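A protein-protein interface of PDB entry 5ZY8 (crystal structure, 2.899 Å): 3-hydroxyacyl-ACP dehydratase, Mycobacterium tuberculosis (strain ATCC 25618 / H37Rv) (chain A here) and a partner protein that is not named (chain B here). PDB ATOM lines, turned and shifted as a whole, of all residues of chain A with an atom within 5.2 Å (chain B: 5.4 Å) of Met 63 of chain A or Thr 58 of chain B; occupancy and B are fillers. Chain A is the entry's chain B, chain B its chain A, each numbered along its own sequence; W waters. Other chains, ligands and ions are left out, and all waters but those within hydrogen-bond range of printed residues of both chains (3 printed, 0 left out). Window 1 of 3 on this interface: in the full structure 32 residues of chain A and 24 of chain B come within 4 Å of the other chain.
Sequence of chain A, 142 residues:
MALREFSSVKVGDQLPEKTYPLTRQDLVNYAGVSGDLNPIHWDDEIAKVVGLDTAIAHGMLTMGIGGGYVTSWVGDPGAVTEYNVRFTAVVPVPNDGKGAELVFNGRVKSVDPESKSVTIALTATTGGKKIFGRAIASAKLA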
ATOM      1  N   GLY A  59      20.102  -4.367  25.326  1.00  0.00           N
ATOM      2  CA  GLY A  59      19.252  -5.343  25.992  1.00  0.00           C
ATOM      3  C   GLY A  59      18.228  -5.931  25.029  1.00  0.00           C
ATOM      4  O   GLY A  59      17.989  -7.145  25.017  1.00  0.00           O
ATOM      5  N   MET A  60      17.643  -5.087  24.171  1.00  0.00           N
ATOM      6  CA  MET A  60      16.623  -5.568  23.257  1.00  0.00           C
ATOM      7  C   MET A  60      17.235  -6.423  22.161  1.00  0.00           C
ATOM      8  O   MET A  60      16.557  -7.304  21.623  1.00  0.00           O
ATOM      9  CB  MET A  60      15.838  -4.402  22.646  1.00  0.00           C
ATOM     10  CG  MET A  60      14.875  -3.677  23.569  1.00  0.00           C
ATOM     11  SD  MET A  60      13.710  -4.854  24.306  1.00  0.00           S
ATOM     12  CE  MET A  60      13.113  -5.756  22.866  1.00  0.00           C
ATOM     13  N   LEU A  61      18.521  -6.226  21.864  1.00  0.00           N
ATOM     14  CA  LEU A  61      19.193  -7.124  20.939  1.00  0.00           C
ATOM     15  C   LEU A  61      19.245  -8.532  21.529  1.00  0.00           C
ATOM     16  O   LEU A  61      18.940  -9.517  20.843  1.00  0.00           O
ATOM     17  CB  LEU A  61      20.588  -6.593  20.613  1.00  0.00           C
ATOM     18  CG  LEU A  61      21.480  -7.566  19.839  1.00  0.00           C
ATOM     19  CD1 LEU A  61      20.765  -8.016  18.582  1.00  0.00           C
ATOM     20  CD2 LEU A  61      22.820  -6.945  19.504  1.00  0.00           C
ATOM     21  N   THR A  62      19.622  -8.655  22.806  1.00  0.00           N
ATOM     22  CA  THR A  62      19.703  -9.993  23.385  1.00  0.00           C
ATOM     23  C   THR A  62      18.302 -10.584  23.553  1.00  0.00           C
ATOM     24  O   THR A  62      18.092 -11.787  23.345  1.00  0.00           O
ATOM     25  CB  THR A  62      20.454  -9.964  24.727  1.00  0.00           C
ATOM     26  OG1 THR A  62      19.767  -9.114  25.651  1.00  0.00           O
ATOM     27  CG2 THR A  62      21.873  -9.434  24.531  1.00  0.00           C
ATOM     28  N   MET A  63      17.314  -9.743  23.874  1.00  0.00           N
ATOM     29  CA  MET A  63      15.947 -10.244  23.926  1.00  0.00           C
ATOM     30  C   MET A  63      15.499 -10.680  22.532  1.00  0.00           C
ATOM     31  O   MET A  63      14.799 -11.691  22.377  1.00  0.00           O
ATOM     32  CB  MET A  63      14.996  -9.198  24.511  1.00  0.00           C
ATOM     33  CG  MET A  63      13.598  -9.764  24.729  1.00  0.00           C
ATOM     34  SD  MET A  63      12.422  -8.632  25.460  1.00  0.00           S
ATOM     35  CE  MET A  63      11.024  -9.708  25.683  1.00  0.00           C
ATOM     36  N   GLY A  64      15.910  -9.931  21.504  1.00  0.00           N
ATOM     37  CA  GLY A  64      15.536 -10.292  20.152  1.00  0.00           C
ATOM     38  C   GLY A  64      16.084 -11.659  19.794  1.00  0.00           C
ATOM     39  O   GLY A  64      15.384 -12.490  19.197  1.00  0.00           O
ATOM     40  N   ILE A  65      17.340 -11.914  20.164  1.00  0.00           N
ATOM     41  CA  ILE A  65      17.936 -13.222  19.919  1.00  0.00           C
ATOM     42  C   ILE A  65      17.130 -14.299  20.634  1.00  0.00           C
ATOM     43  O   ILE A  65      16.859 -15.368  20.074  1.00  0.00           O
ATOM     44  CB  ILE A  65      19.407 -13.232  20.347  1.00  0.00           C
ATOM     45  CG1 ILE A  65      20.202 -12.272  19.468  1.00  0.00           C
ATOM     46  CG2 ILE A  65      19.970 -14.626  20.224  1.00  0.00           C
ATOM     47  CD1 ILE A  65      21.626 -12.059  19.936  1.00  0.00           C
ATOM     48  N   GLY A  66      16.733 -14.040  21.881  1.00  0.00           N
ATOM     49  CA  GLY A  66      15.911 -15.007  22.583  1.00  0.00           C
ATOM     50  C   GLY A  66      14.621 -15.322  21.846  1.00  0.00           C
ATOM     51  O   GLY A  66      14.176 -16.476  21.836  1.00  0.00           O
ATOM     52  N   GLY A  67      14.023 -14.320  21.177  1.00  0.00           N
ATOM     53  CA  GLY A  67      12.780 -14.580  20.470  1.00  0.00           C
ATOM     54  C   GLY A  67      13.007 -15.564  19.344  1.00  0.00           C
ATOM     55  O   GLY A  67      12.195 -16.465  19.118  1.00  0.00           O
ATOM     56  N   TYR A  83       5.987 -13.199  25.909  1.00  0.00           N
ATOM     57  CA  TYR A  83       7.436 -13.326  25.973  1.00  0.00           C
ATOM     58  C   TYR A  83       7.901 -12.220  26.905  1.00  0.00           C
ATOM     59  O   TYR A  83       7.756 -11.034  26.582  1.00  0.00           O
ATOM     60  CB  TYR A  83       8.047 -13.181  24.584  1.00  0.00           C
ATOM     61  CG  TYR A  83       9.552 -13.236  24.525  1.00  0.00           C
ATOM     62  CD1 TYR A  83      10.276 -14.022  25.412  1.00  0.00           C
ATOM     63  CD2 TYR A  83      10.254 -12.497  23.584  1.00  0.00           C
ATOM     64  CE1 TYR A  83      11.655 -14.096  25.337  1.00  0.00           C
ATOM     65  CE2 TYR A  83      11.630 -12.546  23.515  1.00  0.00           C
ATOM     66  CZ  TYR A  83      12.328 -13.349  24.391  1.00  0.00           C
ATOM     67  OH  TYR A  83      13.702 -13.401  24.340  1.00  0.00           O
ATOM     68  N   ASN A  84       8.401 -12.600  28.072  1.00  0.00           N
ATOM     69  CA  ASN A  84       8.714 -11.634  29.109  1.00  0.00           C
ATOM     70  C   ASN A  84      10.140 -11.890  29.590  1.00  0.00           C
ATOM     71  O   ASN A  84      10.466 -13.016  29.990  1.00  0.00           O
ATOM     72  CB  ASN A  84       7.678 -11.755  30.236  1.00  0.00           C
ATOM     73  CG  ASN A  84       7.851 -10.709  31.315  1.00  0.00           C
ATOM     74  OD1 ASN A  84       7.313 -10.857  32.406  1.00  0.00           O
ATOM     75  ND2 ASN A  84       8.558  -9.625  31.002  1.00  0.00           N
ATOM     76  N   VAL A  85      10.964 -10.839  29.632  1.00  0.00           N
ATOM     77  CA  VAL A  85      12.367 -10.965  30.029  1.00  0.00           C
ATOM     78  C   VAL A  85      12.758  -9.822  30.956  1.00  0.00           C
ATOM     79  O   VAL A  85      12.492  -8.651  30.663  1.00  0.00           O
ATOM     80  CB  VAL A  85      13.300 -10.959  28.798  1.00  0.00           C
ATOM     81  CG1 VAL A  85      14.735 -10.878  29.225  1.00  0.00           C
ATOM     82  CG2 VAL A  85      13.094 -12.210  27.958  1.00  0.00           C
ATOM     83  N   PHE A  87      16.024  -7.948  32.634  1.00  0.00           N
ATOM     84  CA  PHE A  87      17.449  -7.727  32.318  1.00  0.00           C
ATOM     85  C   PHE A  87      18.391  -7.534  33.501  1.00  0.00           C
ATOM     86  O   PHE A  87      18.355  -6.495  34.161  1.00  0.00           O
ATOM     87  CB  PHE A  87      17.597  -6.494  31.435  1.00  0.00           C
ATOM     88  CG  PHE A  87      16.822  -6.545  30.192  1.00  0.00           C
ATOM     89  CD1 PHE A  87      17.176  -7.438  29.196  1.00  0.00           C
ATOM     90  CD2 PHE A  87      15.709  -5.744  30.026  1.00  0.00           C
ATOM     91  CE1 PHE A  87      16.471  -7.502  28.027  1.00  0.00           C
ATOM     92  CE2 PHE A  87      14.982  -5.804  28.863  1.00  0.00           C
ATOM     93  CZ  PHE A  87      15.360  -6.688  27.854  1.00  0.00           C
ATOM     94  N   PHE A 132      19.873 -12.534  32.114  1.00  0.00           N
ATOM     95  CA  PHE A 132      18.464 -12.301  32.371  1.00  0.00           C
ATOM     96  C   PHE A 132      18.090 -12.806  33.751  1.00  0.00           C
ATOM     97  O   PHE A 132      18.735 -13.703  34.303  1.00  0.00           O
ATOM     98  CB  PHE A 132      17.546 -13.013  31.358  1.00  0.00           C
ATOM     99  CG  PHE A 132      17.741 -12.589  29.923  1.00  0.00           C
ATOM    100  CD1 PHE A 132      18.153 -11.303  29.602  1.00  0.00           C
ATOM    101  CD2 PHE A 132      17.449 -13.475  28.892  1.00  0.00           C
ATOM    102  CE1 PHE A 132      18.312 -10.922  28.287  1.00  0.00           C
ATOM    103  CE2 PHE A 132      17.590 -13.109  27.560  1.00  0.00           C
ATOM    104  CZ  PHE A 132      18.028 -11.833  27.253  1.00  0.00           C
ATOM    105  N   PHE B  28      15.376  -6.584  10.409  1.00  0.00           N
ATOM    106  CA  PHE B  28      15.334  -6.735  11.863  1.00  0.00           C
ATOM    107  C   PHE B  28      15.522  -8.191  12.274  1.00  0.00           C
ATOM    108  O   PHE B  28      16.309  -8.499  13.177  1.00  0.00           O
ATOM    109  CB  PHE B  28      14.001  -6.190  12.384  1.00  0.00           C
ATOM    110  CG  PHE B  28      13.950  -5.991  13.870  1.00  0.00           C
ATOM    111  CD1 PHE B  28      13.667  -7.060  14.721  1.00  0.00           C
ATOM    112  CD2 PHE B  28      14.164  -4.739  14.427  1.00  0.00           C
ATOM    113  CE1 PHE B  28      13.603  -6.890  16.097  1.00  0.00           C
ATOM    114  CE2 PHE B  28      14.100  -4.567  15.813  1.00  0.00           C
ATOM    115  CZ  PHE B  28      13.818  -5.647  16.644  1.00  0.00           C
ATOM    116  N   VAL B  32      18.697  -9.767  14.665  1.00  0.00           N
ATOM    117  CA  VAL B  32      18.640 -10.481  15.933  1.00  0.00           C
ATOM    118  C   VAL B  32      18.731 -11.990  15.712  1.00  0.00           C
ATOM    119  O   VAL B  32      18.288 -12.771  16.553  1.00  0.00           O
ATOM    120  CB  VAL B  32      17.392 -10.093  16.743  1.00  0.00           C
ATOM    121  CG1 VAL B  32      17.326  -8.592  16.898  1.00  0.00           C
ATOM    122  CG2 VAL B  32      16.107 -10.666  16.117  1.00  0.00           C
ATOM    123  N   PRO B  56       9.395 -10.260  13.671  1.00  0.00           N
ATOM    124  CA  PRO B  56      10.192 -10.731  14.816  1.00  0.00           C
ATOM    125  C   PRO B  56       9.487 -10.391  16.114  1.00  0.00           C
ATOM    126  O   PRO B  56       8.925  -9.304  16.258  1.00  0.00           O
ATOM    127  CB  PRO B  56      11.504  -9.952  14.681  1.00  0.00           C
ATOM    128  CG  PRO B  56      11.573  -9.563  13.226  1.00  0.00           C
ATOM    129  CD  PRO B  56      10.146  -9.352  12.789  1.00  0.00           C
ATOM    130  N   LEU B  57       9.556 -11.303  17.085  1.00  0.00           N
ATOM    131  CA  LEU B  57       8.699 -11.154  18.261  1.00  0.00           C
ATOM    132  C   LEU B  57       8.999  -9.887  19.048  1.00  0.00           C
ATOM    133  O   LEU B  57       8.138  -9.424  19.797  1.00  0.00           O
ATOM    134  CB  LEU B  57       8.838 -12.365  19.189  1.00  0.00           C
ATOM    135  CG  LEU B  57       8.708 -13.748  18.543  1.00  0.00           C
ATOM    136  CD1 LEU B  57       9.215 -14.857  19.456  1.00  0.00           C
ATOM    137  CD2 LEU B  57       7.251 -14.002  18.140  1.00  0.00           C
ATOM    138  N   THR B  58      10.149  -9.262  18.833  1.00  0.00           N
ATOM    139  CA  THR B  58      10.461  -8.013  19.504  1.00  0.00           C
ATOM    140  C   THR B  58      10.318  -6.810  18.592  1.00  0.00           C
ATOM    141  O   THR B  58      10.753  -5.720  18.963  1.00  0.00           O
ATOM    142  CB  THR B  58      11.876  -8.074  20.089  1.00  0.00           C
ATOM    143  OG1 THR B  58      12.810  -8.437  19.067  1.00  0.00           O
ATOM    144  CG2 THR B  58      11.938  -9.097  21.212  1.00  0.00           C
ATOM    145  N   PHE B  59       9.695  -6.979  17.420  1.00  0.00           N
ATOM    146  CA  PHE B  59       9.701  -5.930  16.402  1.00  0.00           C
ATOM    147  C   PHE B  59       9.066  -4.636  16.900  1.00  0.00           C
ATOM    148  O   PHE B  59       9.577  -3.540  16.633  1.00  0.00           O
ATOM    149  CB  PHE B  59       8.970  -6.401  15.159  1.00  0.00           C
ATOM    150  CG  PHE B  59       9.171  -5.503  13.983  1.00  0.00           C
ATOM    151  CD1 PHE B  59      10.413  -5.418  13.370  1.00  0.00           C
ATOM    152  CD2 PHE B  59       8.139  -4.700  13.524  1.00  0.00           C
ATOM    153  CE1 PHE B  59      10.606  -4.586  12.293  1.00  0.00           C
ATOM    154  CE2 PHE B  59       8.330  -3.865  12.466  1.00  0.00           C
ATOM    155  CZ  PHE B  59       9.569  -3.808  11.843  1.00  0.00           C
ATOM    156  N   VAL B  60       7.962  -4.741  17.635  1.00  0.00           N
ATOM    157  CA  VAL B  60       7.172  -3.584  18.043  1.00  0.00           C
ATOM    158  C   VAL B  60       7.929  -2.744  19.076  1.00  0.00           C
ATOM    159  O   VAL B  60       7.472  -1.665  19.476  1.00  0.00           O
ATOM    160  CB  VAL B  60       5.805  -4.070  18.568  1.00  0.00           C
ATOM    161  CG1 VAL B  60       4.909  -2.930  19.047  1.00  0.00           C
ATOM    162  CG2 VAL B  60       5.105  -4.844  17.471  1.00  0.00           C
ATOM    163  N   THR B  61       9.126  -3.191  19.473  1.00  0.00           N
ATOM    164  CA  THR B  61       9.999  -2.306  20.231  1.00  0.00           C
ATOM    165  C   THR B  61      10.241  -0.989  19.504  1.00  0.00           C
ATOM    166  O   THR B  61      10.380   0.058  20.149  1.00  0.00           O
ATOM    167  CB  THR B  61      11.329  -2.981  20.524  1.00  0.00           C
ATOM    168  OG1 THR B  61      12.014  -2.217  21.526  1.00  0.00           O
ATOM    169  CG2 THR B  61      12.192  -3.086  19.253  1.00  0.00           C
ATOM    170  N   ILE B  62      10.293  -1.022  18.170  1.00  0.00           N
ATOM    171  CA  ILE B  62      10.463   0.197  17.385  1.00  0.00           C
ATOM    172  C   ILE B  62       9.294   1.139  17.633  1.00  0.00           C
ATOM    173  O   ILE B  62       9.473   2.333  17.922  1.00  0.00           O
ATOM    174  CB  ILE B  62      10.602  -0.155  15.893  1.00  0.00           C
ATOM    175  CG1 ILE B  62      11.951  -0.819  15.633  1.00  0.00           C
ATOM    176  CG2 ILE B  62      10.425   1.081  15.030  1.00  0.00           C
ATOM    177  CD1 ILE B  62      11.984  -1.692  14.416  1.00  0.00           C
ATOM    178  N   GLN B  89      11.098  -6.156  30.005  1.00  0.00           N
ATOM    179  CA  GLN B  89      10.335  -5.971  28.784  1.00  0.00           C
ATOM    180  C   GLN B  89       9.387  -7.153  28.607  1.00  0.00           C
ATOM    181  O   GLN B  89       9.776  -8.315  28.774  1.00  0.00           O
ATOM    182  CB  GLN B  89      11.278  -5.819  27.577  1.00  0.00           C
ATOM    183  CG  GLN B  89      10.581  -5.629  26.242  1.00  0.00           C
ATOM    184  CD  GLN B  89       9.864  -4.293  26.139  1.00  0.00           C
ATOM    185  OE1 GLN B  89       8.702  -4.237  25.710  1.00  0.00           O
ATOM    186  NE2 GLN B  89      10.554  -3.208  26.517  1.00  0.00           N
ATOM    187  N   ARG B  90       8.142  -6.845  28.248  1.00  0.00           N
ATOM    188  CA  ARG B  90       7.080  -7.834  28.165  1.00  0.00           C
ATOM    189  C   ARG B  90       6.276  -7.626  26.894  1.00  0.00           C
ATOM    190  O   ARG B  90       6.016  -6.484  26.495  1.00  0.00           O
ATOM    191  CB  ARG B  90       6.154  -7.752  29.379  1.00  0.00           C
ATOM    192  CG  ARG B  90       5.206  -8.915  29.457  1.00  0.00           C
ATOM    193  CD  ARG B  90       4.578  -9.042  30.819  1.00  0.00           C
ATOM    194  NE  ARG B  90       3.387  -9.881  30.754  1.00  0.00           N
ATOM    195  CZ  ARG B  90       2.167  -9.469  31.086  1.00  0.00           C
ATOM    196  NH1 ARG B  90       1.986  -8.224  31.531  1.00  0.00           N
ATOM    197  NH2 ARG B  90       1.133 -10.303  30.989  1.00  0.00           N
ATOM    198  N   PHE B  91       5.943  -8.729  26.224  1.00  0.00           N
ATOM    199  CA  PHE B  91       5.077  -8.701  25.053  1.00  0.00           C
ATOM    200  C   PHE B  91       3.945  -9.705  25.239  1.00  0.00           C
ATOM    201  O   PHE B  91       4.197 -10.871  25.571  1.00  0.00           O
ATOM    202  CB  PHE B  91       5.852  -9.043  23.781  1.00  0.00           C
ATOM    203  CG  PHE B  91       6.931  -8.060  23.430  1.00  0.00           C
ATOM    204  CD1 PHE B  91       6.648  -6.941  22.676  1.00  0.00           C
ATOM    205  CD2 PHE B  91       8.242  -8.281  23.819  1.00  0.00           C
ATOM    206  CE1 PHE B  91       7.645  -6.049  22.324  1.00  0.00           C
ATOM    207  CE2 PHE B  91       9.245  -7.390  23.475  1.00  0.00           C
ATOM    208  CZ  PHE B  91       8.944  -6.273  22.729  1.00  0.00           C
HETATM  209  O   HOH W   1      12.949 -11.200  18.276  1.00  0.00           O
HETATM  210  O   HOH W   2      17.340 -15.416  17.574  1.00  0.00           O
HETATM  211  O   HOH W   3      14.935  -6.764  19.431  1.00  0.00           O
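O of Gln 89 of chain B is in hydrogen-bond range of ND2 of Asn 84 of chain A (2.9 Å). The backbone NH (N) of Val 85 of chain A lies within hydrogen-bond range of the backbone carbonyl oxygen (O) of Gln 89 of chain B. O of Tyr 83 of chain A sits at hydrogen-bond distance from N of Phe 91 of chain B.
O of Met 63 of chain A sits at hydrogen-bond distance from OH of Tyr 83 of chain A (2.8 Å). The backbone NH (N) of Gly 67 of chain A sits at hydrogen-bond distance from the side-chain hydroxyl (OH) of Tyr 83 of chain A, at 3.3 Å.
Among the printed residues, pairs that only touch across the chains: Gly 67 of chain A with Leu 57 of chain B (3.4 Å), Ile 65 of chain A with Val 32 of chain B (3.4 Å), Asn 84 of chain A with Arg 90 of chain B (3.5 Å), Gly 64 of chain A with Thr 58 of chain B (3.5 Å), Met 63 of chain A with Gln 89 of chain B (3.6 Å), Tyr 83 of chain A with Arg 90 of chain B (3.6 Å), Met 63 of chain A with Phe 91 of chain B (3.6 Å), Gly 64 of chain A with Val 32 of chain B (3.7 Å), Met 60 of chain A with Gln 89 of chain B (3.8 Å), Met 60 of chain A with Thr 61 of chain B (3.8 Å), Met 60 of chain A with Thr 58 of chain B (3.8 Å), Leu 61 of chain A with Val 32 of chain B (3.9 Å), Phe 87 of chain A with Gln 89 of chain B (3.9 Å) and Met 63 of chain A with Thr 58 of chain B (3.9 Å).
Of chain B, only Thr 58 (3.9 Å), Gln 89 (3.6 Å) and Phe 91 (3.6 Å) come within 4 Å of Met 63 of chain A. Of chain A, only Met 60, Met 63 and Gly 64 come within 4 Å of Thr 58 of chain B. Of the printed residues of chain B, Met 60 of chain A touches Thr 58 (3.8 Å), Thr 61 (3.8 Å) and Gln 89 (3.8 Å). Of the printed residues of chain A, Val 32 of chain B touches Leu 61 (3.9 Å), Gly 64 (3.7 Å) and Ile 65 (3.4 Å). Printed residues of chain A within 4 Å of Thr 61 of chain B: Met 60 (3.8 Å). Of the printed residues of chain B, Gly 67 of chain A touches Leu 57 (3.4 Å). Of the printed residues of chain B, Asn 84 of chain A touches Gln 89 (2.9 Å) and Arg 90 (3.5 Å). The nearest printed residue of chain B that does not touch Met 60 of chain A is Phe 91 of chain B (4.2 Å).
Hydrophobic or aromatic side chains of chain A that line the printed part of chain B: Met 60, Leu 61, Met 63, Ile 65 and Phe 87. Among the printed residues, 17 pairs touch across the chains. Among the printed residues, no Asp or Glu carboxylate lies within 4 Å of a Lys or Arg side-chain nitrogen of the other chain.
Water W2 lies within hydrogen-bond range of the backbone carbonyl oxygen (O) of Ile 65 of chain A and the backbone carbonyl oxygen (O) of Val 32 of chain B. Water W3 lies within hydrogen-bond range of OG1 of Thr 58 of chain B (2.7 Å) and O of Met 60 of chain A (2.8 Å). Water W1 lies within hydrogen-bond range of OG1 of Thr 58 of chain B (2.9 Å) and O of Gly 64 of chain A (2.9 Å).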
